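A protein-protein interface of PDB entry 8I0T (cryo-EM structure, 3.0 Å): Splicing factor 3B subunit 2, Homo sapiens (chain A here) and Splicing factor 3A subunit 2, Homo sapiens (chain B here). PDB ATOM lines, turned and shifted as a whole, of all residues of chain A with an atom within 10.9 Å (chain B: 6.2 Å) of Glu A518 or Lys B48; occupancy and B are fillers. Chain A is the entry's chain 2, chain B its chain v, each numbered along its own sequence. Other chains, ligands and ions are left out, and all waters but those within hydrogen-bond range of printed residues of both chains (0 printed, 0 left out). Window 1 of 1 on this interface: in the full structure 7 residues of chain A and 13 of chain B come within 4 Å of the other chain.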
ATOM      1  N   GLY A 513       8.029  25.970 -25.791  1.00  0.00           N
ATOM      2  CA  GLY A 513       7.907  24.619 -26.300  1.00  0.00           C
ATOM      3  C   GLY A 513       7.725  23.581 -25.216  1.00  0.00           C
ATOM      4  O   GLY A 513       7.290  22.462 -25.496  1.00  0.00           O
ATOM      5  N   LYS A 514       8.110  23.904 -23.984  1.00  0.00           N
ATOM      6  CA  LYS A 514       7.831  23.031 -22.855  1.00  0.00           C
ATOM      7  C   LYS A 514       6.376  23.188 -22.476  1.00  0.00           C
ATOM      8  O   LYS A 514       5.836  22.369 -21.732  1.00  0.00           O
ATOM      9  CB  LYS A 514       8.715  23.350 -21.646  1.00  0.00           C
ATOM     10  CG  LYS A 514      10.166  23.018 -21.815  1.00  0.00           C
ATOM     11  CD  LYS A 514      10.749  22.542 -20.516  1.00  0.00           C
ATOM     12  CE  LYS A 514      11.691  21.400 -20.773  1.00  0.00           C
ATOM     13  NZ  LYS A 514      12.452  20.979 -19.582  1.00  0.00           N
ATOM     14  N   ARG A 515       5.750  24.259 -22.964  1.00  0.00           N
ATOM     15  CA  ARG A 515       4.317  24.475 -22.707  1.00  0.00           C
ATOM     16  C   ARG A 515       3.438  23.224 -22.644  1.00  0.00           C
ATOM     17  O   ARG A 515       2.674  23.053 -21.692  1.00  0.00           O
ATOM     18  CB  ARG A 515       3.703  25.392 -23.770  1.00  0.00           C
ATOM     19  CG  ARG A 515       2.181  25.401 -23.776  1.00  0.00           C
ATOM     20  CD  ARG A 515       1.627  26.461 -24.692  1.00  0.00           C
ATOM     21  NE  ARG A 515       1.767  27.793 -24.120  1.00  0.00           N
ATOM     22  CZ  ARG A 515       1.122  28.868 -24.557  1.00  0.00           C
ATOM     23  NH1 ARG A 515       0.278  28.777 -25.572  1.00  0.00           N
ATOM     24  NH2 ARG A 515       1.314  30.036 -23.969  1.00  0.00           N
ATOM     25  N   GLY A 516       3.518  22.355 -23.648  1.00  0.00           N
ATOM     26  CA  GLY A 516       2.482  21.343 -23.826  1.00  0.00           C
ATOM     27  C   GLY A 516       2.265  20.434 -22.626  1.00  0.00           C
ATOM     28  O   GLY A 516       1.171  20.391 -22.057  1.00  0.00           O
ATOM     29  N   ILE A 517       3.315  19.730 -22.204  1.00  0.00           N
ATOM     30  CA  ILE A 517       3.252  18.486 -21.432  1.00  0.00           C
ATOM     31  C   ILE A 517       2.716  18.641 -20.017  1.00  0.00           C
ATOM     32  O   ILE A 517       2.409  19.749 -19.566  1.00  0.00           O
ATOM     33  CB  ILE A 517       4.640  17.835 -21.353  1.00  0.00           C
ATOM     34  CG1 ILE A 517       5.698  18.789 -21.912  1.00  0.00           C
ATOM     35  CG2 ILE A 517       4.637  16.462 -22.023  1.00  0.00           C
ATOM     36  CD1 ILE A 517       6.466  19.517 -20.840  1.00  0.00           C
ATOM     37  N   GLU A 518       2.547  17.508 -19.334  1.00  0.00           N
ATOM     38  CA  GLU A 518       2.368  17.451 -17.890  1.00  0.00           C
ATOM     39  C   GLU A 518       3.656  16.996 -17.204  1.00  0.00           C
ATOM     40  O   GLU A 518       4.410  16.178 -17.737  1.00  0.00           O
ATOM     41  CB  GLU A 518       1.221  16.510 -17.516  1.00  0.00           C
ATOM     42  CG  GLU A 518       0.828  16.489 -16.033  1.00  0.00           C
ATOM     43  CD  GLU A 518       0.614  17.862 -15.399  1.00  0.00           C
ATOM     44  OE1 GLU A 518       1.557  18.685 -15.352  1.00  0.00           O
ATOM     45  OE2 GLU A 518      -0.510  18.112 -14.913  1.00  0.00           O
ATOM     46  N   LYS A 519       3.886  17.518 -15.994  1.00  0.00           N
ATOM     47  CA  LYS A 519       5.166  17.432 -15.305  1.00  0.00           C
ATOM     48  C   LYS A 519       4.981  17.018 -13.851  1.00  0.00           C
ATOM     49  O   LYS A 519       4.049  17.479 -13.189  1.00  0.00           O
ATOM     50  CB  LYS A 519       5.883  18.792 -15.383  1.00  0.00           C
ATOM     51  CG  LYS A 519       7.193  18.906 -14.632  1.00  0.00           C
ATOM     52  CD  LYS A 519       7.454  20.351 -14.226  1.00  0.00           C
ATOM     53  CE  LYS A 519       8.042  20.449 -12.821  1.00  0.00           C
ATOM     54  NZ  LYS A 519       9.526  20.392 -12.786  1.00  0.00           N
ATOM     55  N   PRO A 520       5.845  16.150 -13.329  1.00  0.00           N
ATOM     56  CA  PRO A 520       5.668  15.645 -11.963  1.00  0.00           C
ATOM     57  C   PRO A 520       6.432  16.477 -10.949  1.00  0.00           C
ATOM     58  O   PRO A 520       7.561  16.908 -11.214  1.00  0.00           O
ATOM     59  CB  PRO A 520       6.233  14.226 -12.051  1.00  0.00           C
ATOM     60  CG  PRO A 520       7.313  14.342 -13.076  1.00  0.00           C
ATOM     61  CD  PRO A 520       6.939  15.455 -14.028  1.00  0.00           C
ATOM     62  N   PRO A 521       5.859  16.692  -9.764  1.00  0.00           N
ATOM     63  CA  PRO A 521       6.474  17.588  -8.780  1.00  0.00           C
ATOM     64  C   PRO A 521       7.897  17.202  -8.407  1.00  0.00           C
ATOM     65  O   PRO A 521       8.348  16.074  -8.610  1.00  0.00           O
ATOM     66  CB  PRO A 521       5.539  17.477  -7.568  1.00  0.00           C
ATOM     67  CG  PRO A 521       4.712  16.292  -7.816  1.00  0.00           C
ATOM     68  CD  PRO A 521       4.555  16.215  -9.294  1.00  0.00           C
ATOM     69  N   PHE A 522       8.603  18.190  -7.857  1.00  0.00           N
ATOM     70  CA  PHE A 522      10.019  18.076  -7.543  1.00  0.00           C
ATOM     71  C   PHE A 522      10.245  16.984  -6.508  1.00  0.00           C
ATOM     72  O   PHE A 522       9.411  16.740  -5.639  1.00  0.00           O
ATOM     73  CB  PHE A 522      10.515  19.445  -7.064  1.00  0.00           C
ATOM     74  CG  PHE A 522      11.790  19.424  -6.291  1.00  0.00           C
ATOM     75  CD1 PHE A 522      11.873  20.072  -5.085  1.00  0.00           C
ATOM     76  CD2 PHE A 522      12.915  18.819  -6.790  1.00  0.00           C
ATOM     77  CE1 PHE A 522      13.030  20.075  -4.378  1.00  0.00           C
ATOM     78  CE2 PHE A 522      14.073  18.811  -6.075  1.00  0.00           C
ATOM     79  CZ  PHE A 522      14.131  19.447  -4.873  1.00  0.00           C
ATOM     80  N   GLU A 596      16.633  16.811 -21.018  1.00  0.00           N
ATOM     81  CA  GLU A 596      16.371  15.717 -20.091  1.00  0.00           C
ATOM     82  C   GLU A 596      15.560  14.613 -20.748  1.00  0.00           C
ATOM     83  O   GLU A 596      15.549  13.482 -20.251  1.00  0.00           O
ATOM     84  CB  GLU A 596      15.657  16.227 -18.844  1.00  0.00           C
ATOM     85  CG  GLU A 596      14.200  16.545 -19.041  1.00  0.00           C
ATOM     86  CD  GLU A 596      13.988  17.846 -19.773  1.00  0.00           C
ATOM     87  OE1 GLU A 596      13.415  18.782 -19.189  1.00  0.00           O
ATOM     88  OE2 GLU A 596      14.400  17.938 -20.942  1.00  0.00           O
ATOM     89  N   PHE A 597      14.879  14.913 -21.857  1.00  0.00           N
ATOM     90  CA  PHE A 597      14.159  13.868 -22.576  1.00  0.00           C
ATOM     91  C   PHE A 597      15.091  13.070 -23.468  1.00  0.00           C
ATOM     92  O   PHE A 597      14.910  11.860 -23.635  1.00  0.00           O
ATOM     93  CB  PHE A 597      13.029  14.468 -23.400  1.00  0.00           C
ATOM     94  CG  PHE A 597      11.912  14.987 -22.573  1.00  0.00           C
ATOM     95  CD1 PHE A 597      11.791  14.608 -21.256  1.00  0.00           C
ATOM     96  CD2 PHE A 597      10.988  15.867 -23.101  1.00  0.00           C
ATOM     97  CE1 PHE A 597      10.772  15.088 -20.481  1.00  0.00           C
ATOM     98  CE2 PHE A 597       9.961  16.353 -22.329  1.00  0.00           C
ATOM     99  CZ  PHE A 597       9.855  15.963 -21.016  1.00  0.00           C
ATOM    100  N   ARG B  31     -13.229  26.939  -8.037  1.00  0.00           N
ATOM    101  CA  ARG B  31     -12.486  25.872  -8.692  1.00  0.00           C
ATOM    102  C   ARG B  31     -13.238  24.555  -8.607  1.00  0.00           C
ATOM    103  O   ARG B  31     -13.259  23.778  -9.565  1.00  0.00           O
ATOM    104  CB  ARG B  31     -11.107  25.746  -8.068  1.00  0.00           C
ATOM    105  CG  ARG B  31     -10.461  24.413  -8.282  1.00  0.00           C
ATOM    106  CD  ARG B  31      -9.179  24.367  -7.508  1.00  0.00           C
ATOM    107  NE  ARG B  31      -8.563  25.689  -7.466  1.00  0.00           N
ATOM    108  CZ  ARG B  31      -7.904  26.166  -6.418  1.00  0.00           C
ATOM    109  NH1 ARG B  31      -7.763  25.420  -5.337  1.00  0.00           N
ATOM    110  NH2 ARG B  31      -7.372  27.379  -6.455  1.00  0.00           N
ATOM    111  N   LEU B  35     -14.509  22.043 -11.507  1.00  0.00           N
ATOM    112  CA  LEU B  35     -14.291  20.608 -11.573  1.00  0.00           C
ATOM    113  C   LEU B  35     -15.610  19.866 -11.716  1.00  0.00           C
ATOM    114  O   LEU B  35     -15.705  18.886 -12.457  1.00  0.00           O
ATOM    115  CB  LEU B  35     -13.526  20.150 -10.342  1.00  0.00           C
ATOM    116  CG  LEU B  35     -12.067  20.594 -10.336  1.00  0.00           C
ATOM    117  CD1 LEU B  35     -11.300  19.812  -9.297  1.00  0.00           C
ATOM    118  CD2 LEU B  35     -11.452  20.416 -11.707  1.00  0.00           C
ATOM    119  N   PHE B  46      -8.686  18.351 -21.223  1.00  0.00           N
ATOM    120  CA  PHE B  46      -8.485  19.191 -20.059  1.00  0.00           C
ATOM    121  C   PHE B  46      -7.218  18.776 -19.336  1.00  0.00           C
ATOM    122  O   PHE B  46      -6.799  17.617 -19.413  1.00  0.00           O
ATOM    123  CB  PHE B  46      -9.677  19.094 -19.127  1.00  0.00           C
ATOM    124  CG  PHE B  46      -9.685  20.113 -18.050  1.00  0.00           C
ATOM    125  CD1 PHE B  46      -9.019  19.900 -16.867  1.00  0.00           C
ATOM    126  CD2 PHE B  46     -10.368  21.288 -18.215  1.00  0.00           C
ATOM    127  CE1 PHE B  46      -9.035  20.850 -15.880  1.00  0.00           C
ATOM    128  CE2 PHE B  46     -10.386  22.238 -17.229  1.00  0.00           C
ATOM    129  CZ  PHE B  46      -9.723  22.021 -16.063  1.00  0.00           C
ATOM    130  N   MET B  47      -6.601  19.743 -18.664  1.00  0.00           N
ATOM    131  CA  MET B  47      -5.476  19.501 -17.780  1.00  0.00           C
ATOM    132  C   MET B  47      -5.414  20.592 -16.725  1.00  0.00           C
ATOM    133  O   MET B  47      -5.741  21.748 -16.987  1.00  0.00           O
ATOM    134  CB  MET B  47      -4.169  19.464 -18.552  1.00  0.00           C
ATOM    135  CG  MET B  47      -2.976  19.087 -17.730  1.00  0.00           C
ATOM    136  SD  MET B  47      -1.765  18.422 -18.857  1.00  0.00           S
ATOM    137  CE  MET B  47      -2.734  17.065 -19.485  1.00  0.00           C
ATOM    138  N   LYS B  48      -4.997  20.215 -15.528  1.00  0.00           N
ATOM    139  CA  LYS B  48      -4.571  21.171 -14.523  1.00  0.00           C
ATOM    140  C   LYS B  48      -3.080  20.969 -14.318  1.00  0.00           C
ATOM    141  O   LYS B  48      -2.647  19.882 -13.926  1.00  0.00           O
ATOM    142  CB  LYS B  48      -5.336  20.987 -13.219  1.00  0.00           C
ATOM    143  CG  LYS B  48      -5.832  22.287 -12.641  1.00  0.00           C
ATOM    144  CD  LYS B  48      -6.492  22.094 -11.287  1.00  0.00           C
ATOM    145  CE  LYS B  48      -6.506  23.392 -10.490  1.00  0.00           C
ATOM    146  NZ  LYS B  48      -6.262  23.164  -9.042  1.00  0.00           N
ATOM    147  N   ASN B  49      -2.298  22.005 -14.594  1.00  0.00           N
ATOM    148  CA  ASN B  49      -0.861  21.852 -14.685  1.00  0.00           C
ATOM    149  C   ASN B  49      -0.247  21.971 -13.303  1.00  0.00           C
ATOM    150  O   ASN B  49      -0.880  22.429 -12.352  1.00  0.00           O
ATOM    151  CB  ASN B  49      -0.281  22.889 -15.635  1.00  0.00           C
ATOM    152  CG  ASN B  49      -0.923  24.220 -15.459  1.00  0.00           C
ATOM    153  OD1 ASN B  49      -1.666  24.425 -14.512  1.00  0.00           O
ATOM    154  ND2 ASN B  49      -0.653  25.139 -16.363  1.00  0.00           N
ATOM    155  N   HIS B  50       1.004  21.583 -13.198  1.00  0.00           N
ATOM    156  CA  HIS B  50       1.735  21.631 -11.948  1.00  0.00           C
ATOM    157  C   HIS B  50       1.857  23.054 -11.369  1.00  0.00           C
ATOM    158  O   HIS B  50       2.512  23.205 -10.345  1.00  0.00           O
ATOM    159  CB  HIS B  50       3.120  21.047 -12.151  1.00  0.00           C
ATOM    160  CG  HIS B  50       4.071  22.009 -12.773  1.00  0.00           C
ATOM    161  ND1 HIS B  50       3.715  22.827 -13.820  1.00  0.00           N
ATOM    162  CD2 HIS B  50       5.349  22.322 -12.468  1.00  0.00           C
ATOM    163  CE1 HIS B  50       4.748  23.576 -14.160  1.00  0.00           C
ATOM    164  NE2 HIS B  50       5.748  23.296 -13.349  1.00  0.00           N
ATOM    165  N   LEU B  51       1.311  24.098 -11.985  1.00  0.00           N
ATOM    166  CA  LEU B  51       1.262  25.420 -11.386  1.00  0.00           C
ATOM    167  C   LEU B  51      -0.150  25.858 -11.042  1.00  0.00           C
ATOM    168  O   LEU B  51      -0.346  27.000 -10.627  1.00  0.00           O
ATOM    169  CB  LEU B  51       1.893  26.453 -12.308  1.00  0.00           C
ATOM    170  CG  LEU B  51       3.267  26.130 -12.862  1.00  0.00           C
ATOM    171  CD1 LEU B  51       3.821  27.327 -13.617  1.00  0.00           C
ATOM    172  CD2 LEU B  51       4.176  25.714 -11.736  1.00  0.00           C
ATOM    173  N   GLY B  52      -1.138  24.991 -11.217  1.00  0.00           N
ATOM    174  CA  GLY B  52      -2.492  25.345 -10.840  1.00  0.00           C
ATOM    175  C   GLY B  52      -3.248  26.199 -11.829  1.00  0.00           C
ATOM    176  O   GLY B  52      -4.229  26.840 -11.453  1.00  0.00           O
ATOM    177  N   SER B  53      -2.829  26.230 -13.078  1.00  0.00           N
ATOM    178  CA  SER B  53      -3.588  26.837 -14.154  1.00  0.00           C
ATOM    179  C   SER B  53      -4.397  25.744 -14.850  1.00  0.00           C
ATOM    180  O   SER B  53      -4.493  24.612 -14.370  1.00  0.00           O
ATOM    181  CB  SER B  53      -2.654  27.559 -15.118  1.00  0.00           C
ATOM    182  OG  SER B  53      -2.403  26.771 -16.265  1.00  0.00           O
ATOM    183  N   TYR B  54      -4.988  26.080 -15.986  1.00  0.00           N
ATOM    184  CA  TYR B  54      -5.708  25.095 -16.766  1.00  0.00           C
ATOM    185  C   TYR B  54      -5.190  25.079 -18.191  1.00  0.00           C
ATOM    186  O   TYR B  54      -4.716  26.090 -18.711  1.00  0.00           O
ATOM    187  CB  TYR B  54      -7.193  25.388 -16.773  1.00  0.00           C
ATOM    188  CG  TYR B  54      -7.736  25.689 -15.417  1.00  0.00           C
ATOM    189  CD1 TYR B  54      -7.616  24.773 -14.401  1.00  0.00           C
ATOM    190  CD2 TYR B  54      -8.384  26.883 -15.154  1.00  0.00           C
ATOM    191  CE1 TYR B  54      -8.116  25.029 -13.160  1.00  0.00           C
ATOM    192  CE2 TYR B  54      -8.887  27.148 -13.916  1.00  0.00           C
ATOM    193  CZ  TYR B  54      -8.748  26.213 -12.918  1.00  0.00           C
ATOM    194  OH  TYR B  54      -9.236  26.455 -11.662  1.00  0.00           O
ATOM    195  N   GLU B  55      -5.300  23.923 -18.827  1.00  0.00           N
ATOM    196  CA  GLU B  55      -4.899  23.765 -20.213  1.00  0.00           C
ATOM    197  C   GLU B  55      -6.068  23.270 -21.040  1.00  0.00           C
ATOM    198  O   GLU B  55      -7.025  22.693 -20.525  1.00  0.00           O
ATOM    199  CB  GLU B  55      -3.763  22.758 -20.409  1.00  0.00           C
ATOM    200  CG  GLU B  55      -2.494  23.022 -19.665  1.00  0.00           C
ATOM    201  CD  GLU B  55      -1.327  22.278 -20.292  1.00  0.00           C
ATOM    202  OE1 GLU B  55      -0.242  22.877 -20.451  1.00  0.00           O
ATOM    203  OE2 GLU B  55      -1.498  21.090 -20.649  1.00  0.00           O
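O of Gly A516 lies close to OE2 of Glu B55 (3.1 Å). O of Lys B48 lies close to OE2 of Glu A518 (2.9 Å). The backbone carbonyl oxygen (O) of Arg A515 sits close to the side-chain carboxylate (OE1) of Glu B55.
OD1 of Asn B49 is in hydrogen-bond range of N of Ser B53 (2.6 Å). The backbone NH of Glu B55 sits at hydrogen-bond distance from the backbone carbonyl oxygen of Met B47 (2.9 Å). The side-chain amide oxygen (OD1) of Asn B49 lies within hydrogen-bond range of the backbone NH (N) of Gly B52 (3.4 Å).
Glu A518 touches Met B47 (CB to SD, 3.8 Å). OE2 of Glu A518 touches CA of Asn B49, 3.8 Å away. Glu A518 touches His B50 (OE1 to N, 3.7 Å). Lys A519 touches His B50 (CE to CD2, 3.3 Å).
Glu A518 touches just these residues of chain B: Met B47 (3.8 Å), Lys B48 (2.9 Å), Asn B49 (3.8 Å) and His B50 (3.7 Å). Lys B48 touches one residue of chain A. Asn B49 touches just one residue of chain A: Glu A518 (3.8 Å). No residue of chain A comes within 4 Å of Ser B53. No residue of chain A comes within 4 Å of Tyr B54. Of chain A, only Arg A515 and Gly A516 come within 4 Å of Glu B55. Of the printed residues of chain B, Gly A516 touches Glu B55. Of the printed residues of chain B, Lys A519 touches His B50 (3.3 Å). Of the printed residues of chain B, Arg A515 touches Glu B55 (3.2 Å). Gly A513 touches none of the printed residues of chain B. Phe A522 touches none of the printed residues of chain B. The nearest residue of chain B that does not touch Glu A518 is Glu B55 (5.6 Å). The nearest printed residue of chain B that does not touch Gly A516 is Met B47 (4.8 Å).
Of the 12 printed residues of chain A, 4 touch a printed residue of chain B. Of the 12 printed residues of chain B, 5 touch a printed residue of chain A. Hydrophobic or aromatic side chains of chain B that line the printed part of chain A: Met B47 and His B50. Among the printed residues, no Asp or Glu carboxylate lies within 4 Å of a Lys or Arg side-chain nitrogen of the other chain.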
